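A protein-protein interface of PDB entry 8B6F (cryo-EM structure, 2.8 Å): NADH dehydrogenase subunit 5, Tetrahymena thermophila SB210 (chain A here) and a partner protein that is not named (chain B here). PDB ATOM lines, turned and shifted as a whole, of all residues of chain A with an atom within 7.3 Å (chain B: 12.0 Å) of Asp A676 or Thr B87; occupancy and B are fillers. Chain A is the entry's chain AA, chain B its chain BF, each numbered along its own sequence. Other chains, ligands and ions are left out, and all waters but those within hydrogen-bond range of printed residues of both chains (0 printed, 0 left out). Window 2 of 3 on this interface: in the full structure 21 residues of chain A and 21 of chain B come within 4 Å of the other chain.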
ATOM      1  N   ILE A 221      -4.439 -14.261 -32.933  1.00  0.00           N
ATOM      2  CA  ILE A 221      -4.143 -15.637 -32.552  1.00  0.00           C
ATOM      3  C   ILE A 221      -2.665 -15.947 -32.756  1.00  0.00           C
ATOM      4  O   ILE A 221      -2.032 -16.596 -31.915  1.00  0.00           O
ATOM      5  CB  ILE A 221      -5.045 -16.609 -33.333  1.00  0.00           C
ATOM      6  CG1 ILE A 221      -6.517 -16.340 -33.013  1.00  0.00           C
ATOM      7  CG2 ILE A 221      -4.701 -18.053 -32.996  1.00  0.00           C
ATOM      8  CD1 ILE A 221      -7.479 -16.980 -33.981  1.00  0.00           C
ATOM      9  N   VAL A 222      -2.093 -15.493 -33.871  1.00  0.00           N
ATOM     10  CA  VAL A 222      -0.729 -15.886 -34.211  1.00  0.00           C
ATOM     11  C   VAL A 222       0.278 -15.234 -33.271  1.00  0.00           C
ATOM     12  O   VAL A 222       1.236 -15.877 -32.830  1.00  0.00           O
ATOM     13  CB  VAL A 222      -0.436 -15.549 -35.684  1.00  0.00           C
ATOM     14  CG1 VAL A 222       1.035 -15.775 -36.014  1.00  0.00           C
ATOM     15  CG2 VAL A 222      -1.314 -16.381 -36.593  1.00  0.00           C
ATOM     16  N   SER A 223       0.086 -13.956 -32.948  1.00  0.00           N
ATOM     17  CA  SER A 223       1.086 -13.189 -32.212  1.00  0.00           C
ATOM     18  C   SER A 223       0.644 -12.779 -30.815  1.00  0.00           C
ATOM     19  O   SER A 223       1.467 -12.768 -29.899  1.00  0.00           O
ATOM     20  CB  SER A 223       1.471 -11.935 -33.006  1.00  0.00           C
ATOM     21  OG  SER A 223       0.338 -11.132 -33.282  1.00  0.00           O
ATOM     22  N   GLU A 224      -0.628 -12.440 -30.617  1.00  0.00           N
ATOM     23  CA  GLU A 224      -1.092 -11.895 -29.345  1.00  0.00           C
ATOM     24  C   GLU A 224      -1.459 -12.964 -28.326  1.00  0.00           C
ATOM     25  O   GLU A 224      -1.907 -12.619 -27.229  1.00  0.00           O
ATOM     26  CB  GLU A 224      -2.300 -10.979 -29.570  1.00  0.00           C
ATOM     27  CG  GLU A 224      -2.036  -9.774 -30.443  1.00  0.00           C
ATOM     28  CD  GLU A 224      -1.109  -8.785 -29.773  1.00  0.00           C
ATOM     29  OE1 GLU A 224      -0.799  -8.976 -28.580  1.00  0.00           O
ATOM     30  OE2 GLU A 224      -0.715  -7.798 -30.421  1.00  0.00           O
ATOM     31  N   ASN A 225      -1.293 -14.243 -28.658  1.00  0.00           N
ATOM     32  CA  ASN A 225      -1.570 -15.341 -27.731  1.00  0.00           C
ATOM     33  C   ASN A 225      -3.060 -15.435 -27.403  1.00  0.00           C
ATOM     34  O   ASN A 225      -3.441 -15.704 -26.265  1.00  0.00           O
ATOM     35  CB  ASN A 225      -0.748 -15.210 -26.446  1.00  0.00           C
ATOM     36  CG  ASN A 225       0.744 -15.277 -26.698  1.00  0.00           C
ATOM     37  OD1 ASN A 225       1.324 -16.358 -26.776  1.00  0.00           O
ATOM     38  ND2 ASN A 225       1.375 -14.115 -26.821  1.00  0.00           N
ATOM     39  N   TYR A 227      -6.460 -17.527 -28.070  1.00  0.00           N
ATOM     40  CA  TYR A 227      -7.109 -18.714 -28.601  1.00  0.00           C
ATOM     41  C   TYR A 227      -8.396 -18.940 -27.828  1.00  0.00           C
ATOM     42  O   TYR A 227      -8.510 -18.556 -26.662  1.00  0.00           O
ATOM     43  CB  TYR A 227      -6.204 -19.952 -28.539  1.00  0.00           C
ATOM     44  CG  TYR A 227      -5.764 -20.366 -27.157  1.00  0.00           C
ATOM     45  CD1 TYR A 227      -6.565 -21.177 -26.365  1.00  0.00           C
ATOM     46  CD2 TYR A 227      -4.531 -19.973 -26.659  1.00  0.00           C
ATOM     47  CE1 TYR A 227      -6.159 -21.569 -25.105  1.00  0.00           C
ATOM     48  CE2 TYR A 227      -4.115 -20.358 -25.401  1.00  0.00           C
ATOM     49  CZ  TYR A 227      -4.932 -21.156 -24.629  1.00  0.00           C
ATOM     50  OH  TYR A 227      -4.519 -21.541 -23.376  1.00  0.00           O
ATOM     51  N   ASP A 251      -7.081 -22.249 -31.991  1.00  0.00           N
ATOM     52  CA  ASP A 251      -5.745 -22.029 -31.462  1.00  0.00           C
ATOM     53  C   ASP A 251      -4.821 -21.623 -32.607  1.00  0.00           C
ATOM     54  O   ASP A 251      -5.258 -21.427 -33.743  1.00  0.00           O
ATOM     55  CB  ASP A 251      -5.247 -23.292 -30.753  1.00  0.00           C
ATOM     56  CG  ASP A 251      -4.124 -23.013 -29.774  1.00  0.00           C
ATOM     57  OD1 ASP A 251      -3.399 -22.017 -29.968  1.00  0.00           O
ATOM     58  OD2 ASP A 251      -3.966 -23.790 -28.809  1.00  0.00           O
ATOM     59  N   LEU A 252      -3.530 -21.483 -32.302  1.00  0.00           N
ATOM     60  CA  LEU A 252      -2.569 -21.200 -33.362  1.00  0.00           C
ATOM     61  C   LEU A 252      -2.504 -22.350 -34.358  1.00  0.00           C
ATOM     62  O   LEU A 252      -2.454 -22.128 -35.572  1.00  0.00           O
ATOM     63  CB  LEU A 252      -1.186 -20.919 -32.773  1.00  0.00           C
ATOM     64  CG  LEU A 252      -0.078 -20.646 -33.799  1.00  0.00           C
ATOM     65  CD1 LEU A 252       0.939 -19.679 -33.237  1.00  0.00           C
ATOM     66  CD2 LEU A 252       0.625 -21.920 -34.244  1.00  0.00           C
ATOM     67  N   THR A 253      -2.486 -23.588 -33.862  1.00  0.00           N
ATOM     68  CA  THR A 253      -2.426 -24.733 -34.762  1.00  0.00           C
ATOM     69  C   THR A 253      -3.645 -24.771 -35.673  1.00  0.00           C
ATOM     70  O   THR A 253      -3.524 -25.037 -36.874  1.00  0.00           O
ATOM     71  CB  THR A 253      -2.317 -26.030 -33.957  1.00  0.00           C
ATOM     72  OG1 THR A 253      -1.091 -26.035 -33.213  1.00  0.00           O
ATOM     73  CG2 THR A 253      -2.345 -27.247 -34.876  1.00  0.00           C
ATOM     74  N   ASN A 371      -2.132 -32.994 -22.612  1.00  0.00           N
ATOM     75  CA  ASN A 371      -1.519 -32.765 -21.314  1.00  0.00           C
ATOM     76  C   ASN A 371      -1.497 -33.999 -20.423  1.00  0.00           C
ATOM     77  O   ASN A 371      -0.889 -33.952 -19.350  1.00  0.00           O
ATOM     78  CB  ASN A 371      -2.248 -31.629 -20.591  1.00  0.00           C
ATOM     79  CG  ASN A 371      -2.136 -30.310 -21.327  1.00  0.00           C
ATOM     80  OD1 ASN A 371      -3.134 -29.739 -21.759  1.00  0.00           O
ATOM     81  ND2 ASN A 371      -0.912 -29.821 -21.478  1.00  0.00           N
ATOM     82  N   TYR A 672      11.631 -13.040 -31.198  1.00  0.00           N
ATOM     83  CA  TYR A 672      10.651 -14.092 -31.431  1.00  0.00           C
ATOM     84  C   TYR A 672       9.306 -13.663 -30.860  1.00  0.00           C
ATOM     85  O   TYR A 672       9.173 -13.476 -29.646  1.00  0.00           O
ATOM     86  CB  TYR A 672      11.131 -15.393 -30.791  1.00  0.00           C
ATOM     87  CG  TYR A 672      10.230 -16.579 -31.031  1.00  0.00           C
ATOM     88  CD1 TYR A 672      10.385 -17.379 -32.154  1.00  0.00           C
ATOM     89  CD2 TYR A 672       9.233 -16.906 -30.124  1.00  0.00           C
ATOM     90  CE1 TYR A 672       9.568 -18.468 -32.369  1.00  0.00           C
ATOM     91  CE2 TYR A 672       8.411 -17.992 -30.330  1.00  0.00           C
ATOM     92  CZ  TYR A 672       8.583 -18.768 -31.454  1.00  0.00           C
ATOM     93  OH  TYR A 672       7.760 -19.851 -31.660  1.00  0.00           O
ATOM     94  N   SER A 673       8.308 -13.512 -31.732  1.00  0.00           N
ATOM     95  CA  SER A 673       7.004 -12.990 -31.342  1.00  0.00           C
ATOM     96  C   SER A 673       5.863 -13.929 -31.717  1.00  0.00           C
ATOM     97  O   SER A 673       4.708 -13.499 -31.770  1.00  0.00           O
ATOM     98  CB  SER A 673       6.775 -11.614 -31.968  1.00  0.00           C
ATOM     99  OG  SER A 673       6.789 -11.694 -33.382  1.00  0.00           O
ATOM    100  N   LEU A 674       6.154 -15.197 -31.985  1.00  0.00           N
ATOM    101  CA  LEU A 674       5.102 -16.157 -32.278  1.00  0.00           C
ATOM    102  C   LEU A 674       4.384 -16.555 -30.995  1.00  0.00           C
ATOM    103  O   LEU A 674       4.949 -16.505 -29.899  1.00  0.00           O
ATOM    104  CB  LEU A 674       5.675 -17.398 -32.961  1.00  0.00           C
ATOM    105  CG  LEU A 674       4.660 -18.344 -33.608  1.00  0.00           C
ATOM    106  CD1 LEU A 674       4.015 -17.704 -34.826  1.00  0.00           C
ATOM    107  CD2 LEU A 674       5.309 -19.665 -33.979  1.00  0.00           C
ATOM    108  N   SER A 675       3.122 -16.944 -31.137  1.00  0.00           N
ATOM    109  CA  SER A 675       2.348 -17.372 -29.985  1.00  0.00           C
ATOM    110  C   SER A 675       2.821 -18.744 -29.512  1.00  0.00           C
ATOM    111  O   SER A 675       3.556 -19.457 -30.198  1.00  0.00           O
ATOM    112  CB  SER A 675       0.859 -17.413 -30.317  1.00  0.00           C
ATOM    113  OG  SER A 675       0.360 -16.115 -30.578  1.00  0.00           O
ATOM    114  N   ASP A 676       2.384 -19.109 -28.310  1.00  0.00           N
ATOM    115  CA  ASP A 676       2.804 -20.366 -27.712  1.00  0.00           C
ATOM    116  C   ASP A 676       2.306 -21.546 -28.537  1.00  0.00           C
ATOM    117  O   ASP A 676       1.157 -21.573 -28.984  1.00  0.00           O
ATOM    118  CB  ASP A 676       2.266 -20.456 -26.286  1.00  0.00           C
ATOM    119  CG  ASP A 676       2.824 -21.634 -25.522  1.00  0.00           C
ATOM    120  OD1 ASP A 676       3.741 -22.307 -26.036  1.00  0.00           O
ATOM    121  OD2 ASP A 676       2.329 -21.890 -24.405  1.00  0.00           O
ATOM    122  N   LEU A 677       3.185 -22.526 -28.741  1.00  0.00           N
ATOM    123  CA  LEU A 677       2.838 -23.742 -29.464  1.00  0.00           C
ATOM    124  C   LEU A 677       2.398 -24.878 -28.551  1.00  0.00           C
ATOM    125  O   LEU A 677       1.987 -25.930 -29.051  1.00  0.00           O
ATOM    126  CB  LEU A 677       4.034 -24.203 -30.301  1.00  0.00           C
ATOM    127  CG  LEU A 677       4.422 -23.286 -31.461  1.00  0.00           C
ATOM    128  CD1 LEU A 677       5.790 -23.658 -31.985  1.00  0.00           C
ATOM    129  CD2 LEU A 677       3.390 -23.367 -32.565  1.00  0.00           C
ATOM    130  N   LYS A 678       2.473 -24.693 -27.234  1.00  0.00           N
ATOM    131  CA  LYS A 678       2.025 -25.693 -26.268  1.00  0.00           C
ATOM    132  C   LYS A 678       2.829 -26.987 -26.373  1.00  0.00           C
ATOM    133  O   LYS A 678       2.296 -28.078 -26.161  1.00  0.00           O
ATOM    134  CB  LYS A 678       0.531 -25.983 -26.434  1.00  0.00           C
ATOM    135  CG  LYS A 678      -0.341 -24.734 -26.494  1.00  0.00           C
ATOM    136  CD  LYS A 678      -0.189 -23.878 -25.244  1.00  0.00           C
ATOM    137  CE  LYS A 678      -1.064 -22.636 -25.316  1.00  0.00           C
ATOM    138  NZ  LYS A 678      -0.939 -21.792 -24.096  1.00  0.00           N
ATOM    139  N   SER A 679       4.118 -26.879 -26.691  1.00  0.00           N
ATOM    140  CA  SER A 679       5.015 -28.024 -26.755  1.00  0.00           C
ATOM    141  C   SER A 679       6.258 -27.727 -25.932  1.00  0.00           C
ATOM    142  O   SER A 679       6.782 -26.610 -25.972  1.00  0.00           O
ATOM    143  CB  SER A 679       5.410 -28.353 -28.197  1.00  0.00           C
ATOM    144  OG  SER A 679       6.137 -27.286 -28.781  1.00  0.00           O
ATOM    145  N   ILE A 680       6.732 -28.729 -25.192  1.00  0.00           N
ATOM    146  CA  ILE A 680       7.888 -28.568 -24.318  1.00  0.00           C
ATOM    147  C   ILE A 680       9.139 -29.220 -24.900  1.00  0.00           C
ATOM    148  O   ILE A 680      10.128 -29.396 -24.184  1.00  0.00           O
ATOM    149  CB  ILE A 680       7.602 -29.111 -22.909  1.00  0.00           C
ATOM    150  CG1 ILE A 680       7.392 -30.628 -22.953  1.00  0.00           C
ATOM    151  CG2 ILE A 680       6.383 -28.411 -22.318  1.00  0.00           C
ATOM    152  CD1 ILE A 680       7.169 -31.260 -21.599  1.00  0.00           C
ATOM    153  N   VAL B  78      -8.248 -30.874 -15.949  1.00  0.00           N
ATOM    154  CA  VAL B  78      -7.017 -30.804 -16.731  1.00  0.00           C
ATOM    155  C   VAL B  78      -7.199 -29.883 -17.928  1.00  0.00           C
ATOM    156  O   VAL B  78      -6.305 -29.101 -18.271  1.00  0.00           O
ATOM    157  CB  VAL B  78      -6.584 -32.214 -17.171  1.00  0.00           C
ATOM    158  CG1 VAL B  78      -5.427 -32.147 -18.158  1.00  0.00           C
ATOM    159  CG2 VAL B  78      -6.188 -33.031 -15.979  1.00  0.00           C
ATOM    160  N   ARG B  79      -8.352 -29.969 -18.596  1.00  0.00           N
ATOM    161  CA  ARG B  79      -8.628 -29.051 -19.695  1.00  0.00           C
ATOM    162  C   ARG B  79      -8.653 -27.611 -19.203  1.00  0.00           C
ATOM    163  O   ARG B  79      -8.119 -26.712 -19.861  1.00  0.00           O
ATOM    164  CB  ARG B  79      -9.953 -29.415 -20.362  1.00  0.00           C
ATOM    165  CG  ARG B  79     -10.411 -28.416 -21.413  1.00  0.00           C
ATOM    166  CD  ARG B  79     -11.713 -28.855 -22.050  1.00  0.00           C
ATOM    167  NE  ARG B  79     -12.793 -28.953 -21.076  1.00  0.00           N
ATOM    168  CZ  ARG B  79     -13.954 -29.551 -21.303  1.00  0.00           C
ATOM    169  NH1 ARG B  79     -14.221 -30.126 -22.464  1.00  0.00           N
ATOM    170  NH2 ARG B  79     -14.872 -29.572 -20.340  1.00  0.00           N
ATOM    171  N   ARG B  80      -9.282 -27.373 -18.051  1.00  0.00           N
ATOM    172  CA  ARG B  80      -9.315 -26.028 -17.488  1.00  0.00           C
ATOM    173  C   ARG B  80      -7.909 -25.530 -17.188  1.00  0.00           C
ATOM    174  O   ARG B  80      -7.573 -24.376 -17.478  1.00  0.00           O
ATOM    175  CB  ARG B  80     -10.174 -26.020 -16.223  1.00  0.00           C
ATOM    176  CG  ARG B  80     -10.128 -24.723 -15.428  1.00  0.00           C
ATOM    177  CD  ARG B  80     -10.863 -24.876 -14.111  1.00  0.00           C
ATOM    178  NE  ARG B  80     -12.298 -25.050 -14.310  1.00  0.00           N
ATOM    179  CZ  ARG B  80     -13.185 -24.065 -14.316  1.00  0.00           C
ATOM    180  NH1 ARG B  80     -12.826 -22.807 -14.129  1.00  0.00           N
ATOM    181  NH2 ARG B  80     -14.468 -24.353 -14.508  1.00  0.00           N
ATOM    182  N   ALA B  81      -7.070 -26.389 -16.609  1.00  0.00           N
ATOM    183  CA  ALA B  81      -5.689 -26.012 -16.340  1.00  0.00           C
ATOM    184  C   ALA B  81      -4.947 -25.690 -17.628  1.00  0.00           C
ATOM    185  O   ALA B  81      -4.188 -24.717 -17.690  1.00  0.00           O
ATOM    186  CB  ALA B  81      -4.980 -27.132 -15.582  1.00  0.00           C
ATOM    187  N   ALA B  82      -5.150 -26.498 -18.669  1.00  0.00           N
ATOM    188  CA  ALA B  82      -4.473 -26.246 -19.936  1.00  0.00           C
ATOM    189  C   ALA B  82      -4.863 -24.894 -20.518  1.00  0.00           C
ATOM    190  O   ALA B  82      -4.008 -24.161 -21.029  1.00  0.00           O
ATOM    191  CB  ALA B  82      -4.796 -27.366 -20.924  1.00  0.00           C
ATOM    192  N   ILE B  83      -6.149 -24.549 -20.465  1.00  0.00           N
ATOM    193  CA  ILE B  83      -6.593 -23.283 -21.041  1.00  0.00           C
ATOM    194  C   ILE B  83      -6.103 -22.107 -20.202  1.00  0.00           C
ATOM    195  O   ILE B  83      -5.626 -21.103 -20.742  1.00  0.00           O
ATOM    196  CB  ILE B  83      -8.125 -23.282 -21.217  1.00  0.00           C
ATOM    197  CG1 ILE B  83      -8.508 -24.328 -22.271  1.00  0.00           C
ATOM    198  CG2 ILE B  83      -8.629 -21.894 -21.607  1.00  0.00           C
ATOM    199  CD1 ILE B  83      -9.985 -24.472 -22.522  1.00  0.00           C
ATOM    200  N   LEU B  84      -6.218 -22.203 -18.877  1.00  0.00           N
ATOM    201  CA  LEU B  84      -5.887 -21.062 -18.028  1.00  0.00           C
ATOM    202  C   LEU B  84      -4.380 -20.836 -17.961  1.00  0.00           C
ATOM    203  O   LEU B  84      -3.907 -19.702 -18.100  1.00  0.00           O
ATOM    204  CB  LEU B  84      -6.458 -21.271 -16.624  1.00  0.00           C
ATOM    205  CG  LEU B  84      -7.984 -21.276 -16.500  1.00  0.00           C
ATOM    206  CD1 LEU B  84      -8.397 -21.621 -15.081  1.00  0.00           C
ATOM    207  CD2 LEU B  84      -8.577 -19.940 -16.917  1.00  0.00           C
ATOM    208  N   THR B  85      -3.608 -21.902 -17.748  1.00  0.00           N
ATOM    209  CA  THR B  85      -2.177 -21.763 -17.490  1.00  0.00           C
ATOM    210  C   THR B  85      -1.388 -21.916 -18.785  1.00  0.00           C
ATOM    211  O   THR B  85      -1.648 -22.849 -19.553  1.00  0.00           O
ATOM    212  CB  THR B  85      -1.705 -22.802 -16.481  1.00  0.00           C
ATOM    213  OG1 THR B  85      -2.481 -22.701 -15.282  1.00  0.00           O
ATOM    214  CG2 THR B  85      -0.235 -22.601 -16.141  1.00  0.00           C
ATOM    215  N   PRO B  86      -0.422 -21.041 -19.066  1.00  0.00           N
ATOM    216  CA  PRO B  86       0.399 -21.219 -20.268  1.00  0.00           C
ATOM    217  C   PRO B  86       1.269 -22.461 -20.157  1.00  0.00           C
ATOM    218  O   PRO B  86       1.518 -22.987 -19.072  1.00  0.00           O
ATOM    219  CB  PRO B  86       1.246 -19.942 -20.317  1.00  0.00           C
ATOM    220  CG  PRO B  86       1.296 -19.472 -18.912  1.00  0.00           C
ATOM    221  CD  PRO B  86      -0.022 -19.846 -18.302  1.00  0.00           C
ATOM    222  N   THR B  87       1.737 -22.931 -21.317  1.00  0.00           N
ATOM    223  CA  THR B  87       2.486 -24.183 -21.350  1.00  0.00           C
ATOM    224  C   THR B  87       3.681 -24.146 -20.407  1.00  0.00           C
ATOM    225  O   THR B  87       4.077 -25.186 -19.868  1.00  0.00           O
ATOM    226  CB  THR B  87       2.940 -24.490 -22.778  1.00  0.00           C
ATOM    227  OG1 THR B  87       3.270 -25.879 -22.887  1.00  0.00           O
ATOM    228  CG2 THR B  87       4.171 -23.674 -23.157  1.00  0.00           C
ATOM    229  N   SER B  88       4.267 -22.971 -20.198  1.00  0.00           N
ATOM    230  CA  SER B  88       5.318 -22.831 -19.202  1.00  0.00           C
ATOM    231  C   SER B  88       4.709 -22.902 -17.809  1.00  0.00           C
ATOM    232  O   SER B  88       3.745 -22.196 -17.504  1.00  0.00           O
ATOM    233  CB  SER B  88       6.064 -21.512 -19.395  1.00  0.00           C
ATOM    234  OG  SER B  88       5.194 -20.405 -19.233  1.00  0.00           O
ATOM    235  N   SER B  89       5.270 -23.761 -16.964  1.00  0.00           N
ATOM    236  CA  SER B  89       4.817 -24.031 -15.606  1.00  0.00           C
ATOM    237  C   SER B  89       3.564 -24.900 -15.591  1.00  0.00           C
ATOM    238  O   SER B  89       3.102 -25.261 -14.504  1.00  0.00           O
ATOM    239  CB  SER B  89       4.535 -22.748 -14.809  1.00  0.00           C
ATOM    240  OG  SER B  89       3.427 -22.045 -15.343  1.00  0.00           O
ATOM    241  N   LEU B  90       2.988 -25.238 -16.747  1.00  0.00           N
ATOM    242  CA  LEU B  90       1.792 -26.073 -16.754  1.00  0.00           C
ATOM    243  C   LEU B  90       2.090 -27.460 -16.197  1.00  0.00           C
ATOM    244  O   LEU B  90       1.365 -27.962 -15.331  1.00  0.00           O
ATOM    245  CB  LEU B  90       1.225 -26.168 -18.170  1.00  0.00           C
ATOM    246  CG  LEU B  90       0.022 -27.101 -18.350  1.00  0.00           C
ATOM    247  CD1 LEU B  90      -1.075 -26.792 -17.346  1.00  0.00           C
ATOM    248  CD2 LEU B  90      -0.515 -26.999 -19.765  1.00  0.00           C
ATOM    249  N   ARG B  91       3.155 -28.102 -16.686  1.00  0.00           N
ATOM    250  CA  ARG B  91       3.522 -29.410 -16.153  1.00  0.00           C
ATOM    251  C   ARG B  91       4.025 -29.311 -14.722  1.00  0.00           C
ATOM    252  O   ARG B  91       3.814 -30.235 -13.928  1.00  0.00           O
ATOM    253  CB  ARG B  91       4.576 -30.074 -17.036  1.00  0.00           C
ATOM    254  CG  ARG B  91       4.014 -30.668 -18.313  1.00  0.00           C
ATOM    255  CD  ARG B  91       4.886 -31.797 -18.831  1.00  0.00           C
ATOM    256  NE  ARG B  91       4.346 -32.371 -20.058  1.00  0.00           N
ATOM    257  CZ  ARG B  91       4.880 -33.397 -20.706  1.00  0.00           C
ATOM    258  NH1 ARG B  91       5.969 -34.003 -20.264  1.00  0.00           N
ATOM    259  NH2 ARG B  91       4.310 -33.821 -21.831  1.00  0.00           N
ATOM    260  N   GLU B  92       4.692 -28.211 -14.371  1.00  0.00           N
ATOM    261  CA  GLU B  92       5.131 -28.036 -12.991  1.00  0.00           C
ATOM    262  C   GLU B  92       3.940 -28.018 -12.046  1.00  0.00           C
ATOM    263  O   GLU B  92       3.973 -28.639 -10.978  1.00  0.00           O
ATOM    264  CB  GLU B  92       5.941 -26.747 -12.848  1.00  0.00           C
ATOM    265  CG  GLU B  92       7.334 -26.800 -13.464  1.00  0.00           C
ATOM    266  CD  GLU B  92       7.315 -26.781 -14.982  1.00  0.00           C
ATOM    267  OE1 GLU B  92       6.214 -26.814 -15.569  1.00  0.00           O
ATOM    268  OE2 GLU B  92       8.405 -26.730 -15.589  1.00  0.00           O
ATOM    269  N   LYS B  93       2.874 -27.312 -12.426  1.00  0.00           N
ATOM    270  CA  LYS B  93       1.680 -27.260 -11.594  1.00  0.00           C
ATOM    271  C   LYS B  93       0.875 -28.548 -11.672  1.00  0.00           C
ATOM    272  O   LYS B  93       0.168 -28.890 -10.718  1.00  0.00           O
ATOM    273  CB  LYS B  93       0.818 -26.067 -12.003  1.00  0.00           C
ATOM    274  CG  LYS B  93       1.500 -24.724 -11.792  1.00  0.00           C
ATOM    275  CD  LYS B  93       0.631 -23.578 -12.274  1.00  0.00           C
ATOM    276  CE  LYS B  93       1.311 -22.240 -12.040  1.00  0.00           C
ATOM    277  NZ  LYS B  93       0.463 -21.103 -12.491  1.00  0.00           N
ATOM    278  N   MET B  94       0.959 -29.272 -12.791  1.00  0.00           N
ATOM    279  CA  MET B  94       0.250 -30.541 -12.902  1.00  0.00           C
ATOM    280  C   MET B  94       0.928 -31.648 -12.110  1.00  0.00           C
ATOM    281  O   MET B  94       0.252 -32.575 -11.655  1.00  0.00           O
ATOM    282  CB  MET B  94       0.128 -30.962 -14.366  1.00  0.00           C
ATOM    283  CG  MET B  94      -0.955 -30.222 -15.131  1.00  0.00           C
ATOM    284  SD  MET B  94      -1.224 -30.887 -16.785  1.00  0.00           S
ATOM    285  CE  MET B  94      -1.798 -32.544 -16.410  1.00  0.00           C
ATOM    286  N   ASN B  95       2.247 -31.578 -11.929  1.00  0.00           N
ATOM    287  CA  ASN B  95       2.944 -32.585 -11.140  1.00  0.00           C
ATOM    288  C   ASN B  95       2.633 -32.359  -9.668  1.00  0.00           C
ATOM    289  O   ASN B  95       3.518 -32.041  -8.868  1.00  0.00           O
ATOM    290  CB  ASN B  95       4.449 -32.530 -11.395  1.00  0.00           C
ATOM    291  CG  ASN B  95       4.804 -32.842 -12.832  1.00  0.00           C
ATOM    292  OD1 ASN B  95       4.072 -33.545 -13.524  1.00  0.00           O
ATOM    293  ND2 ASN B  95       5.934 -32.316 -13.289  1.00  0.00           N
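The backbone NH (N) of Thr B87 lies close to the side-chain carboxylate (OD2) of Asp A676. The side-chain hydroxyl (OH) of Tyr A227 sits at hydrogen-bond distance from the backbone carbonyl oxygen (O) of Ile B83 (2.9 Å).
Of the 19 printed residues of chain A, 5 touch a printed residue of chain B. Hydrophobic or aromatic side chains of chain A that line the printed part of chain B: Tyr A227 and Ile A680.
Glu A224 touches none of the printed residues of chain B. No residue of chain B comes within 4 Å of Asn A225. Asp A251 touches none of the printed residues of chain B. No residue of chain B comes within 4 Å of Leu A252. Of the printed residues of chain B, Asn A371 touches Ala B82, Leu B90 and Met B94. No residue of chain B comes within 4 Å of Leu A674. Printed residues of chain B within 4 Å of Asp A676: Thr B87 (2.9 Å). No residue of chain B comes within 4 Å of Leu A677. Of chain B, only Thr B87 comes within 4 Å of Lys A678. No residue of chain B comes within 4 Å of Ser A679. Thr B87 touches just these residues of chain A: Asp A676 and Lys A678. Of the printed residues of chain A, Leu B90 touches Asn A371. Of the printed residues of chain A, Met B94 touches Asn A371 (3.4 Å).
The side-chain carboxylate of Asp A676 is in salt-bridge range of the side-chain amino group of Lys A678, 3.3 Å away. OD1 of Asn A225 is in hydrogen-bond range of N of Asp A676, 3.3 Å away. The side-chain amide nitrogen of Asn B95 sits close to the backbone carbonyl oxygen of Arg B91 (3.0 Å).
Ala B82 touches Tyr A227. Asn A371 touches Ala B82 (OD1 to CB, 3.0 Å). CD2 of Leu B90 touches ND2 of Asn A371, 3.3 Å away. O of Asn A371 touches CE of Met B94, at 3.4 Å. Thr B87 touches Lys A678 (OG1 to CA, 3.6 Å). Arg B91 touches Ile A680 (CZ to CD1, 3.3 Å).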
